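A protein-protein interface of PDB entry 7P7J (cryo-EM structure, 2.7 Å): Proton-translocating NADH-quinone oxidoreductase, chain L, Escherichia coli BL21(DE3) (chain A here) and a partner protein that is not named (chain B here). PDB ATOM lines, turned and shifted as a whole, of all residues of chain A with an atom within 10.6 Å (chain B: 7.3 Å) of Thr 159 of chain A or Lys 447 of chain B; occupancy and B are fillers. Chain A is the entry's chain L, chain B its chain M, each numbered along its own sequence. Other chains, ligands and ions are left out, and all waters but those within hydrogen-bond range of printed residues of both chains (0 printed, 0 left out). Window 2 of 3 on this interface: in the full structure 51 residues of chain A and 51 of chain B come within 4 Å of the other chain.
The backbone NH (N) of Gly 446 of chain B is in hydrogen-bond range of the backbone carbonyl oxygen (O) of Tyr 158 of chain A (2.8 Å).
O of Gly 376 of chain B lies within hydrogen-bond range of OG of Ser 379 of chain B (3.3 Å).
N of Gly 376 of chain B sits at hydrogen-bond distance from O of Phe 445 of chain B (3.4 Å).
Among the printed residues, pairs that only touch across the chains: Tyr 158 of chain A with Ser 379 of chain B, Tyr 158 of chain A with Phe 445 of chain B, Thr 159 of chain A with Gly 446 of chain B, Thr 159 of chain A with Lys 447 of chain B, Pro 161 of chain A with His 441 of chain B and Gly 164 of chain A with His 441 of chain B.
Printed residues of chain B within 4 Å of Tyr 158 of chain A: Ser 379, Phe 445 and Gly 446.
Printed residues of chain B within 4 Å of Thr 159 of chain A: Gly 446 (3.6 Å) and Lys 447 (3.6 Å).
No residue of chain A comes within 4 Å of Gly 376 of chain B.
Of the printed residues of chain A, Ser 379 of chain B touches Tyr 158.
Printed residues of chain A within 4 Å of Gly 446 of chain B: Tyr 158 (2.8 Å) and Thr 159 (3.6 Å).
Lys 447 of chain B touches just one residue of chain A: Thr 159 (3.6 Å).
No residue of chain A comes within 4 Å of Ala 448 of chain B.
The nearest residue of chain A that does not touch Lys 447 of chain B is Asp 160 of chain A (5.0 Å).
Printed residues of chain A that touch a printed residue of chain B: Tyr 158, Thr 159, Pro 161 and Gly 164.
Printed residues of chain B that touch a printed residue of chain A: Ser 379, His 441, Phe 445, Gly 446 and Lys 447.
Hydrophobic or aromatic side chains of chain B that line the printed part of chain A: His 441 and Phe 445.
Along chain B the printed residues that touch a printed residue of chain A span positions 379 to 447.
Among the printed residues, 7 pairs touch across the chains.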
ATOM      1  N   GLU A 110      -9.296  -3.973 -34.729  1.00  0.00           N
ATOM      2  CA  GLU A 110      -8.592  -3.166 -33.744  1.00  0.00           C
ATOM      3  C   GLU A 110      -7.571  -2.281 -34.443  1.00  0.00           C
ATOM      4  O   GLU A 110      -6.877  -2.726 -35.362  1.00  0.00           O
ATOM      5  CB  GLU A 110      -7.891  -4.048 -32.708  1.00  0.00           C
ATOM      6  CG  GLU A 110      -8.827  -4.940 -31.915  1.00  0.00           C
ATOM      7  CD  GLU A 110      -9.700  -4.160 -30.953  1.00  0.00           C
ATOM      8  OE1 GLU A 110      -9.234  -3.127 -30.428  1.00  0.00           O
ATOM      9  OE2 GLU A 110     -10.854  -4.578 -30.723  1.00  0.00           O
ATOM     10  N   GLU A 111      -7.497  -1.024 -34.015  1.00  0.00           N
ATOM     11  CA  GLU A 111      -6.477  -0.122 -34.532  1.00  0.00           C
ATOM     12  C   GLU A 111      -5.101  -0.567 -34.056  1.00  0.00           C
ATOM     13  O   GLU A 111      -4.943  -1.063 -32.938  1.00  0.00           O
ATOM     14  CB  GLU A 111      -6.754   1.311 -34.086  1.00  0.00           C
ATOM     15  CG  GLU A 111      -7.495   1.421 -32.766  1.00  0.00           C
ATOM     16  CD  GLU A 111      -7.477   2.829 -32.205  1.00  0.00           C
ATOM     17  OE1 GLU A 111      -6.914   3.726 -32.867  1.00  0.00           O
ATOM     18  OE2 GLU A 111      -8.028   3.041 -31.104  1.00  0.00           O
ATOM     19  N   GLY A 112      -4.101  -0.387 -34.911  1.00  0.00           N
ATOM     20  CA  GLY A 112      -2.778  -0.887 -34.604  1.00  0.00           C
ATOM     21  C   GLY A 112      -2.611  -2.368 -34.846  1.00  0.00           C
ATOM     22  O   GLY A 112      -1.799  -3.009 -34.176  1.00  0.00           O
ATOM     23  N   ARG A 115       0.770  -2.764 -36.408  1.00  0.00           N
ATOM     24  CA  ARG A 115       1.741  -2.447 -35.365  1.00  0.00           C
ATOM     25  C   ARG A 115       1.858  -3.581 -34.354  1.00  0.00           C
ATOM     26  O   ARG A 115       2.966  -3.930 -33.927  1.00  0.00           O
ATOM     27  CB  ARG A 115       1.344  -1.143 -34.674  1.00  0.00           C
ATOM     28  CG  ARG A 115       2.176  -0.789 -33.463  1.00  0.00           C
ATOM     29  CD  ARG A 115       1.851   0.604 -32.974  1.00  0.00           C
ATOM     30  NE  ARG A 115       0.413   0.830 -32.913  1.00  0.00           N
ATOM     31  CZ  ARG A 115      -0.297   0.830 -31.795  1.00  0.00           C
ATOM     32  NH1 ARG A 115       0.268   0.627 -30.617  1.00  0.00           N
ATOM     33  NH2 ARG A 115      -1.609   1.038 -31.860  1.00  0.00           N
ATOM     34  N   LEU A 152       6.918  -2.650 -25.597  1.00  0.00           N
ATOM     35  CA  LEU A 152       6.078  -2.161 -26.687  1.00  0.00           C
ATOM     36  C   LEU A 152       4.738  -2.879 -26.743  1.00  0.00           C
ATOM     37  O   LEU A 152       3.758  -2.317 -27.242  1.00  0.00           O
ATOM     38  CB  LEU A 152       6.803  -2.312 -28.022  1.00  0.00           C
ATOM     39  CG  LEU A 152       7.944  -1.336 -28.287  1.00  0.00           C
ATOM     40  CD1 LEU A 152       8.656  -1.684 -29.579  1.00  0.00           C
ATOM     41  CD2 LEU A 152       7.418   0.079 -28.330  1.00  0.00           C
ATOM     42  N   ILE A 154       3.170  -4.632 -23.917  1.00  0.00           N
ATOM     43  CA  ILE A 154       2.358  -4.485 -22.712  1.00  0.00           C
ATOM     44  C   ILE A 154       1.553  -3.194 -22.775  1.00  0.00           C
ATOM     45  O   ILE A 154       0.341  -3.183 -22.528  1.00  0.00           O
ATOM     46  CB  ILE A 154       3.244  -4.544 -21.455  1.00  0.00           C
ATOM     47  CG1 ILE A 154       3.658  -5.983 -21.165  1.00  0.00           C
ATOM     48  CG2 ILE A 154       2.523  -3.970 -20.252  1.00  0.00           C
ATOM     49  CD1 ILE A 154       4.931  -6.095 -20.375  1.00  0.00           C
ATOM     50  N   GLY A 155       2.202  -2.095 -23.138  1.00  0.00           N
ATOM     51  CA  GLY A 155       1.509  -0.835 -23.298  1.00  0.00           C
ATOM     52  C   GLY A 155       1.028  -0.632 -24.717  1.00  0.00           C
ATOM     53  O   GLY A 155       1.234   0.436 -25.300  1.00  0.00           O
ATOM     54  N   PHE A 156       0.391  -1.658 -25.285  1.00  0.00           N
ATOM     55  CA  PHE A 156      -0.064  -1.582 -26.669  1.00  0.00           C
ATOM     56  C   PHE A 156      -1.211  -0.594 -26.816  1.00  0.00           C
ATOM     57  O   PHE A 156      -1.209   0.243 -27.725  1.00  0.00           O
ATOM     58  CB  PHE A 156      -0.477  -2.965 -27.164  1.00  0.00           C
ATOM     59  CG  PHE A 156      -1.105  -2.951 -28.522  1.00  0.00           C
ATOM     60  CD1 PHE A 156      -0.340  -2.694 -29.646  1.00  0.00           C
ATOM     61  CD2 PHE A 156      -2.460  -3.183 -28.676  1.00  0.00           C
ATOM     62  CE1 PHE A 156      -0.916  -2.673 -30.895  1.00  0.00           C
ATOM     63  CE2 PHE A 156      -3.040  -3.165 -29.922  1.00  0.00           C
ATOM     64  CZ  PHE A 156      -2.268  -2.910 -31.032  1.00  0.00           C
ATOM     65  N   TYR A 157      -2.201  -0.672 -25.932  1.00  0.00           N
ATOM     66  CA  TYR A 157      -3.282   0.310 -25.904  1.00  0.00           C
ATOM     67  C   TYR A 157      -2.744   1.547 -25.203  1.00  0.00           C
ATOM     68  O   TYR A 157      -2.903   1.728 -23.996  1.00  0.00           O
ATOM     69  CB  TYR A 157      -4.511  -0.245 -25.199  1.00  0.00           C
ATOM     70  CG  TYR A 157      -5.064  -1.505 -25.815  1.00  0.00           C
ATOM     71  CD1 TYR A 157      -5.563  -1.506 -27.108  1.00  0.00           C
ATOM     72  CD2 TYR A 157      -5.095  -2.692 -25.099  1.00  0.00           C
ATOM     73  CE1 TYR A 157      -6.073  -2.656 -27.673  1.00  0.00           C
ATOM     74  CE2 TYR A 157      -5.602  -3.844 -25.654  1.00  0.00           C
ATOM     75  CZ  TYR A 157      -6.089  -3.823 -26.940  1.00  0.00           C
ATOM     76  OH  TYR A 157      -6.595  -4.973 -27.494  1.00  0.00           O
ATOM     77  N   TYR A 158      -2.092   2.413 -25.980  1.00  0.00           N
ATOM     78  CA  TYR A 158      -1.387   3.556 -25.415  1.00  0.00           C
ATOM     79  C   TYR A 158      -2.317   4.655 -24.924  1.00  0.00           C
ATOM     80  O   TYR A 158      -1.841   5.582 -24.263  1.00  0.00           O
ATOM     81  CB  TYR A 158      -0.411   4.129 -26.444  1.00  0.00           C
ATOM     82  CG  TYR A 158      -1.018   4.466 -27.788  1.00  0.00           C
ATOM     83  CD1 TYR A 158      -1.569   5.717 -28.031  1.00  0.00           C
ATOM     84  CD2 TYR A 158      -1.016   3.541 -28.823  1.00  0.00           C
ATOM     85  CE1 TYR A 158      -2.117   6.028 -29.257  1.00  0.00           C
ATOM     86  CE2 TYR A 158      -1.561   3.844 -30.050  1.00  0.00           C
ATOM     87  CZ  TYR A 158      -2.109   5.088 -30.263  1.00  0.00           C
ATOM     88  OH  TYR A 158      -2.653   5.393 -31.488  1.00  0.00           O
ATOM     89  N   THR A 159      -3.613   4.586 -25.235  1.00  0.00           N
ATOM     90  CA  THR A 159      -4.538   5.629 -24.802  1.00  0.00           C
ATOM     91  C   THR A 159      -4.743   5.598 -23.294  1.00  0.00           C
ATOM     92  O   THR A 159      -4.895   6.650 -22.662  1.00  0.00           O
ATOM     93  CB  THR A 159      -5.875   5.482 -25.527  1.00  0.00           C
ATOM     94  OG1 THR A 159      -6.464   4.220 -25.193  1.00  0.00           O
ATOM     95  CG2 THR A 159      -5.671   5.555 -27.030  1.00  0.00           C
ATOM     96  N   ASP A 160      -4.751   4.413 -22.701  1.00  0.00           N
ATOM     97  CA  ASP A 160      -4.876   4.290 -21.255  1.00  0.00           C
ATOM     98  C   ASP A 160      -3.511   4.484 -20.607  1.00  0.00           C
ATOM     99  O   ASP A 160      -2.580   3.733 -20.918  1.00  0.00           O
ATOM    100  CB  ASP A 160      -5.445   2.928 -20.885  1.00  0.00           C
ATOM    101  CG  ASP A 160      -5.852   2.838 -19.428  1.00  0.00           C
ATOM    102  OD1 ASP A 160      -5.996   3.893 -18.777  1.00  0.00           O
ATOM    103  OD2 ASP A 160      -6.030   1.707 -18.929  1.00  0.00           O
ATOM    104  N   PRO A 161      -3.341   5.475 -19.725  1.00  0.00           N
ATOM    105  CA  PRO A 161      -2.037   5.656 -19.066  1.00  0.00           C
ATOM    106  C   PRO A 161      -1.655   4.527 -18.123  1.00  0.00           C
ATOM    107  O   PRO A 161      -0.468   4.401 -17.799  1.00  0.00           O
ATOM    108  CB  PRO A 161      -2.207   6.979 -18.308  1.00  0.00           C
ATOM    109  CG  PRO A 161      -3.330   7.674 -19.002  1.00  0.00           C
ATOM    110  CD  PRO A 161      -4.259   6.588 -19.436  1.00  0.00           C
ATOM    111  N   LYS A 162      -2.613   3.716 -17.665  1.00  0.00           N
ATOM    112  CA  LYS A 162      -2.280   2.587 -16.802  1.00  0.00           C
ATOM    113  C   LYS A 162      -1.449   1.549 -17.544  1.00  0.00           C
ATOM    114  O   LYS A 162      -0.508   0.981 -16.977  1.00  0.00           O
ATOM    115  CB  LYS A 162      -3.554   1.953 -16.249  1.00  0.00           C
ATOM    116  CG  LYS A 162      -4.268   2.798 -15.197  1.00  0.00           C
ATOM    117  CD  LYS A 162      -5.125   2.002 -14.187  1.00  0.00           C
ATOM    118  CE  LYS A 162      -5.873   0.745 -14.695  1.00  0.00           C
ATOM    119  NZ  LYS A 162      -6.481   0.751 -16.067  1.00  0.00           N
ATOM    120  N   ASN A 163      -1.781   1.293 -18.812  1.00  0.00           N
ATOM    121  CA  ASN A 163      -0.996   0.363 -19.618  1.00  0.00           C
ATOM    122  C   ASN A 163       0.413   0.888 -19.851  1.00  0.00           C
ATOM    123  O   ASN A 163       1.382   0.122 -19.821  1.00  0.00           O
ATOM    124  CB  ASN A 163      -1.698   0.107 -20.949  1.00  0.00           C
ATOM    125  CG  ASN A 163      -3.184  -0.108 -20.788  1.00  0.00           C
ATOM    126  OD1 ASN A 163      -3.671  -0.352 -19.686  1.00  0.00           O
ATOM    127  ND2 ASN A 163      -3.915  -0.018 -21.890  1.00  0.00           N
ATOM    128  N   GLY A 164       0.546   2.197 -20.078  1.00  0.00           N
ATOM    129  CA  GLY A 164       1.866   2.781 -20.239  1.00  0.00           C
ATOM    130  C   GLY A 164       2.691   2.721 -18.968  1.00  0.00           C
ATOM    131  O   GLY A 164       3.895   2.455 -19.014  1.00  0.00           O
ATOM    132  N   ALA A 165       2.055   2.956 -17.819  1.00  0.00           N
ATOM    133  CA  ALA A 165       2.754   2.843 -16.542  1.00  0.00           C
ATOM    134  C   ALA A 165       3.185   1.406 -16.272  1.00  0.00           C
ATOM    135  O   ALA A 165       4.289   1.168 -15.768  1.00  0.00           O
ATOM    136  CB  ALA A 165       1.869   3.360 -15.411  1.00  0.00           C
ATOM    137  N   ALA A 244      -1.784  -5.756 -17.809  1.00  0.00           N
ATOM    138  CA  ALA A 244      -2.686  -4.776 -18.401  1.00  0.00           C
ATOM    139  C   ALA A 244      -2.752  -4.851 -19.924  1.00  0.00           C
ATOM    140  O   ALA A 244      -3.613  -4.195 -20.517  1.00  0.00           O
ATOM    141  CB  ALA A 244      -2.274  -3.365 -17.977  1.00  0.00           C
ATOM    142  N   MET B 374       1.118  18.293 -24.612  1.00  0.00           N
ATOM    143  CA  MET B 374       0.944  17.305 -25.664  1.00  0.00           C
ATOM    144  C   MET B 374       0.828  15.919 -25.053  1.00  0.00           C
ATOM    145  O   MET B 374       1.301  15.660 -23.946  1.00  0.00           O
ATOM    146  CB  MET B 374       2.093  17.336 -26.682  1.00  0.00           C
ATOM    147  CG  MET B 374       3.470  17.036 -26.117  1.00  0.00           C
ATOM    148  SD  MET B 374       4.736  17.364 -27.357  1.00  0.00           S
ATOM    149  CE  MET B 374       6.140  17.823 -26.360  1.00  0.00           C
ATOM    150  N   GLY B 375       0.183  15.028 -25.795  1.00  0.00           N
ATOM    151  CA  GLY B 375      -0.018  13.665 -25.350  1.00  0.00           C
ATOM    152  C   GLY B 375      -0.874  12.892 -26.325  1.00  0.00           C
ATOM    153  O   GLY B 375      -1.761  13.466 -26.963  1.00  0.00           O
ATOM    154  N   GLY B 376      -0.622  11.593 -26.452  1.00  0.00           N
ATOM    155  CA  GLY B 376      -1.363  10.785 -27.405  1.00  0.00           C
ATOM    156  C   GLY B 376      -1.117  11.183 -28.843  1.00  0.00           C
ATOM    157  O   GLY B 376      -2.040  11.142 -29.665  1.00  0.00           O
ATOM    158  N   LEU B 377       0.112  11.572 -29.164  1.00  0.00           N
ATOM    159  CA  LEU B 377       0.450  12.019 -30.507  1.00  0.00           C
ATOM    160  C   LEU B 377       0.734  10.871 -31.459  1.00  0.00           C
ATOM    161  O   LEU B 377       1.002  11.123 -32.637  1.00  0.00           O
ATOM    162  CB  LEU B 377       1.657  12.958 -30.460  1.00  0.00           C
ATOM    163  CG  LEU B 377       1.400  14.363 -29.918  1.00  0.00           C
ATOM    164  CD1 LEU B 377       2.708  15.055 -29.605  1.00  0.00           C
ATOM    165  CD2 LEU B 377       0.597  15.174 -30.913  1.00  0.00           C
ATOM    166  N   SER B 379      -1.456   8.651 -32.474  1.00  0.00           N
ATOM    167  CA  SER B 379      -2.606   8.549 -33.363  1.00  0.00           C
ATOM    168  C   SER B 379      -2.804   9.781 -34.235  1.00  0.00           C
ATOM    169  O   SER B 379      -3.584   9.719 -35.191  1.00  0.00           O
ATOM    170  CB  SER B 379      -3.872   8.299 -32.543  1.00  0.00           C
ATOM    171  OG  SER B 379      -4.007   9.266 -31.517  1.00  0.00           O
ATOM    172  N   HIS B 441       6.425   8.469 -22.894  1.00  0.00           N
ATOM    173  CA  HIS B 441       5.087   8.416 -22.319  1.00  0.00           C
ATOM    174  C   HIS B 441       4.456   9.798 -22.249  1.00  0.00           C
ATOM    175  O   HIS B 441       3.253   9.949 -22.488  1.00  0.00           O
ATOM    176  CB  HIS B 441       5.141   7.783 -20.931  1.00  0.00           C
ATOM    177  CG  HIS B 441       3.796   7.570 -20.314  1.00  0.00           C
ATOM    178  ND1 HIS B 441       3.266   8.426 -19.372  1.00  0.00           N
ATOM    179  CD2 HIS B 441       2.870   6.602 -20.507  1.00  0.00           C
ATOM    180  CE1 HIS B 441       2.072   7.991 -19.009  1.00  0.00           C
ATOM    181  NE2 HIS B 441       1.809   6.886 -19.683  1.00  0.00           N
ATOM    182  N   ARG B 442       5.246  10.821 -21.922  1.00  0.00           N
ATOM    183  CA  ARG B 442       4.699  12.164 -21.801  1.00  0.00           C
ATOM    184  C   ARG B 442       4.437  12.824 -23.145  1.00  0.00           C
ATOM    185  O   ARG B 442       3.634  13.759 -23.208  1.00  0.00           O
ATOM    186  CB  ARG B 442       5.641  13.044 -20.978  1.00  0.00           C
ATOM    187  CG  ARG B 442       5.682  12.695 -19.504  1.00  0.00           C
ATOM    188  CD  ARG B 442       6.278  13.824 -18.691  1.00  0.00           C
ATOM    189  NE  ARG B 442       7.722  13.923 -18.856  1.00  0.00           N
ATOM    190  CZ  ARG B 442       8.605  13.612 -17.917  1.00  0.00           C
ATOM    191  NH1 ARG B 442       8.225  13.163 -16.734  1.00  0.00           N
ATOM    192  NH2 ARG B 442       9.901  13.764 -18.171  1.00  0.00           N
ATOM    193  N   ALA B 443       5.082  12.368 -24.220  1.00  0.00           N
ATOM    194  CA  ALA B 443       4.943  13.026 -25.515  1.00  0.00           C
ATOM    195  C   ALA B 443       3.902  12.362 -26.413  1.00  0.00           C
ATOM    196  O   ALA B 443       2.951  13.016 -26.846  1.00  0.00           O
ATOM    197  CB  ALA B 443       6.302  13.074 -26.223  1.00  0.00           C
ATOM    198  N   TYR B 444       4.061  11.070 -26.702  1.00  0.00           N
ATOM    199  CA  TYR B 444       3.284  10.417 -27.747  1.00  0.00           C
ATOM    200  C   TYR B 444       2.268   9.406 -27.239  1.00  0.00           C
ATOM    201  O   TYR B 444       1.504   8.870 -28.048  1.00  0.00           O
ATOM    202  CB  TYR B 444       4.222   9.718 -28.740  1.00  0.00           C
ATOM    203  CG  TYR B 444       5.348  10.600 -29.212  1.00  0.00           C
ATOM    204  CD1 TYR B 444       5.126  11.597 -30.150  1.00  0.00           C
ATOM    205  CD2 TYR B 444       6.631  10.446 -28.713  1.00  0.00           C
ATOM    206  CE1 TYR B 444       6.149  12.410 -30.579  1.00  0.00           C
ATOM    207  CE2 TYR B 444       7.662  11.256 -29.135  1.00  0.00           C
ATOM    208  CZ  TYR B 444       7.414  12.236 -30.070  1.00  0.00           C
ATOM    209  OH  TYR B 444       8.436  13.048 -30.498  1.00  0.00           O
ATOM    210  N   PHE B 445       2.232   9.125 -25.943  1.00  0.00           N
ATOM    211  CA  PHE B 445       1.323   8.136 -25.393  1.00  0.00           C
ATOM    212  C   PHE B 445       0.353   8.803 -24.428  1.00  0.00           C
ATOM    213  O   PHE B 445       0.641   9.853 -23.849  1.00  0.00           O
ATOM    214  CB  PHE B 445       2.084   7.012 -24.680  1.00  0.00           C
ATOM    215  CG  PHE B 445       2.971   6.211 -25.587  1.00  0.00           C
ATOM    216  CD1 PHE B 445       2.611   5.979 -26.902  1.00  0.00           C
ATOM    217  CD2 PHE B 445       4.166   5.691 -25.125  1.00  0.00           C
ATOM    218  CE1 PHE B 445       3.424   5.245 -27.738  1.00  0.00           C
ATOM    219  CE2 PHE B 445       4.984   4.955 -25.957  1.00  0.00           C
ATOM    220  CZ  PHE B 445       4.611   4.733 -27.266  1.00  0.00           C
ATOM    221  N   GLY B 446      -0.809   8.178 -24.265  1.00  0.00           N
ATOM    222  CA  GLY B 446      -1.841   8.716 -23.402  1.00  0.00           C
ATOM    223  C   GLY B 446      -2.954   9.377 -24.184  1.00  0.00           C
ATOM    224  O   GLY B 446      -3.239   8.993 -25.321  1.00  0.00           O
ATOM    225  N   LYS B 447      -3.596  10.369 -23.581  1.00  0.00           N
ATOM    226  CA  LYS B 447      -4.623  11.159 -24.238  1.00  0.00           C
ATOM    227  C   LYS B 447      -4.101  12.567 -24.491  1.00  0.00           C
ATOM    228  O   LYS B 447      -3.047  12.966 -23.990  1.00  0.00           O
ATOM    229  CB  LYS B 447      -5.901  11.202 -23.394  1.00  0.00           C
ATOM    230  CG  LYS B 447      -6.499   9.837 -23.111  1.00  0.00           C
ATOM    231  CD  LYS B 447      -7.324   9.849 -21.835  1.00  0.00           C
ATOM    232  CE  LYS B 447      -8.249   8.643 -21.753  1.00  0.00           C
ATOM    233  NZ  LYS B 447      -8.311   7.880 -23.030  1.00  0.00           N
ATOM    234  N   ALA B 448      -4.855  13.319 -25.286  1.00  0.00           N
ATOM    235  CA  ALA B 448      -4.486  14.695 -25.589  1.00  0.00           C
ATOM    236  C   ALA B 448      -4.687  15.564 -24.355  1.00  0.00           C
ATOM    237  O   ALA B 448      -5.811  15.710 -23.865  1.00  0.00           O
ATOM    238  CB  ALA B 448      -5.312  15.220 -26.760  1.00  0.00           C
ATOM    239  N   LYS B 449      -3.599  16.136 -23.851  1.00  0.00           N
ATOM    240  CA  LYS B 449      -3.652  16.987 -22.671  1.00  0.00           C
ATOM    241  C   LYS B 449      -3.957  18.441 -23.005  1.00  0.00           C
ATOM    242  O   LYS B 449      -4.038  19.267 -22.090  1.00  0.00           O
ATOM    243  CB  LYS B 449      -2.337  16.892 -21.893  1.00  0.00           C
ATOM    244  CG  LYS B 449      -2.109  15.532 -21.253  1.00  0.00           C
ATOM    245  CD  LYS B 449      -1.029  15.584 -20.186  1.00  0.00           C
ATOM    246  CE  LYS B 449       0.357  15.613 -20.797  1.00  0.00           C
ATOM    247  NZ  LYS B 449       0.655  14.365 -21.548  1.00  0.00           N
ATOM    248  N   SER B 450      -4.123  18.771 -24.281  1.00  0.00           N
ATOM    249  CA  SER B 450      -4.505  20.114 -24.697  1.00  0.00           C
ATOM    250  C   SER B 450      -5.291  20.005 -25.999  1.00  0.00           C
ATOM    251  O   SER B 450      -5.616  18.906 -26.458  1.00  0.00           O
ATOM    252  CB  SER B 450      -3.271  21.012 -24.840  1.00  0.00           C
ATOM    253  OG  SER B 450      -2.496  20.625 -25.958  1.00  0.00           O
ATOM    254  N   ALA B 453      -3.032  19.134 -29.679  1.00  0.00           N
ATOM    255  CA  ALA B 453      -2.755  17.736 -29.972  1.00  0.00           C
ATOM    256  C   ALA B 453      -4.019  16.917 -30.187  1.00  0.00           C
ATOM    257  O   ALA B 453      -3.924  15.716 -30.457  1.00  0.00           O
ATOM    258  CB  ALA B 453      -1.925  17.117 -28.842  1.00  0.00           C
ATOM    259  N   SER B 454      -5.195  17.533 -30.071  1.00  0.00           N
ATOM    260  CA  SER B 454      -6.447  16.803 -30.239  1.00  0.00           C
ATOM    261  C   SER B 454      -6.766  16.528 -31.702  1.00  0.00           C
ATOM    262  O   SER B 454      -7.352  15.486 -32.016  1.00  0.00           O
ATOM    263  CB  SER B 454      -7.595  17.575 -29.591  1.00  0.00           C
ATOM    264  OG  SER B 454      -7.370  17.752 -28.202  1.00  0.00           O
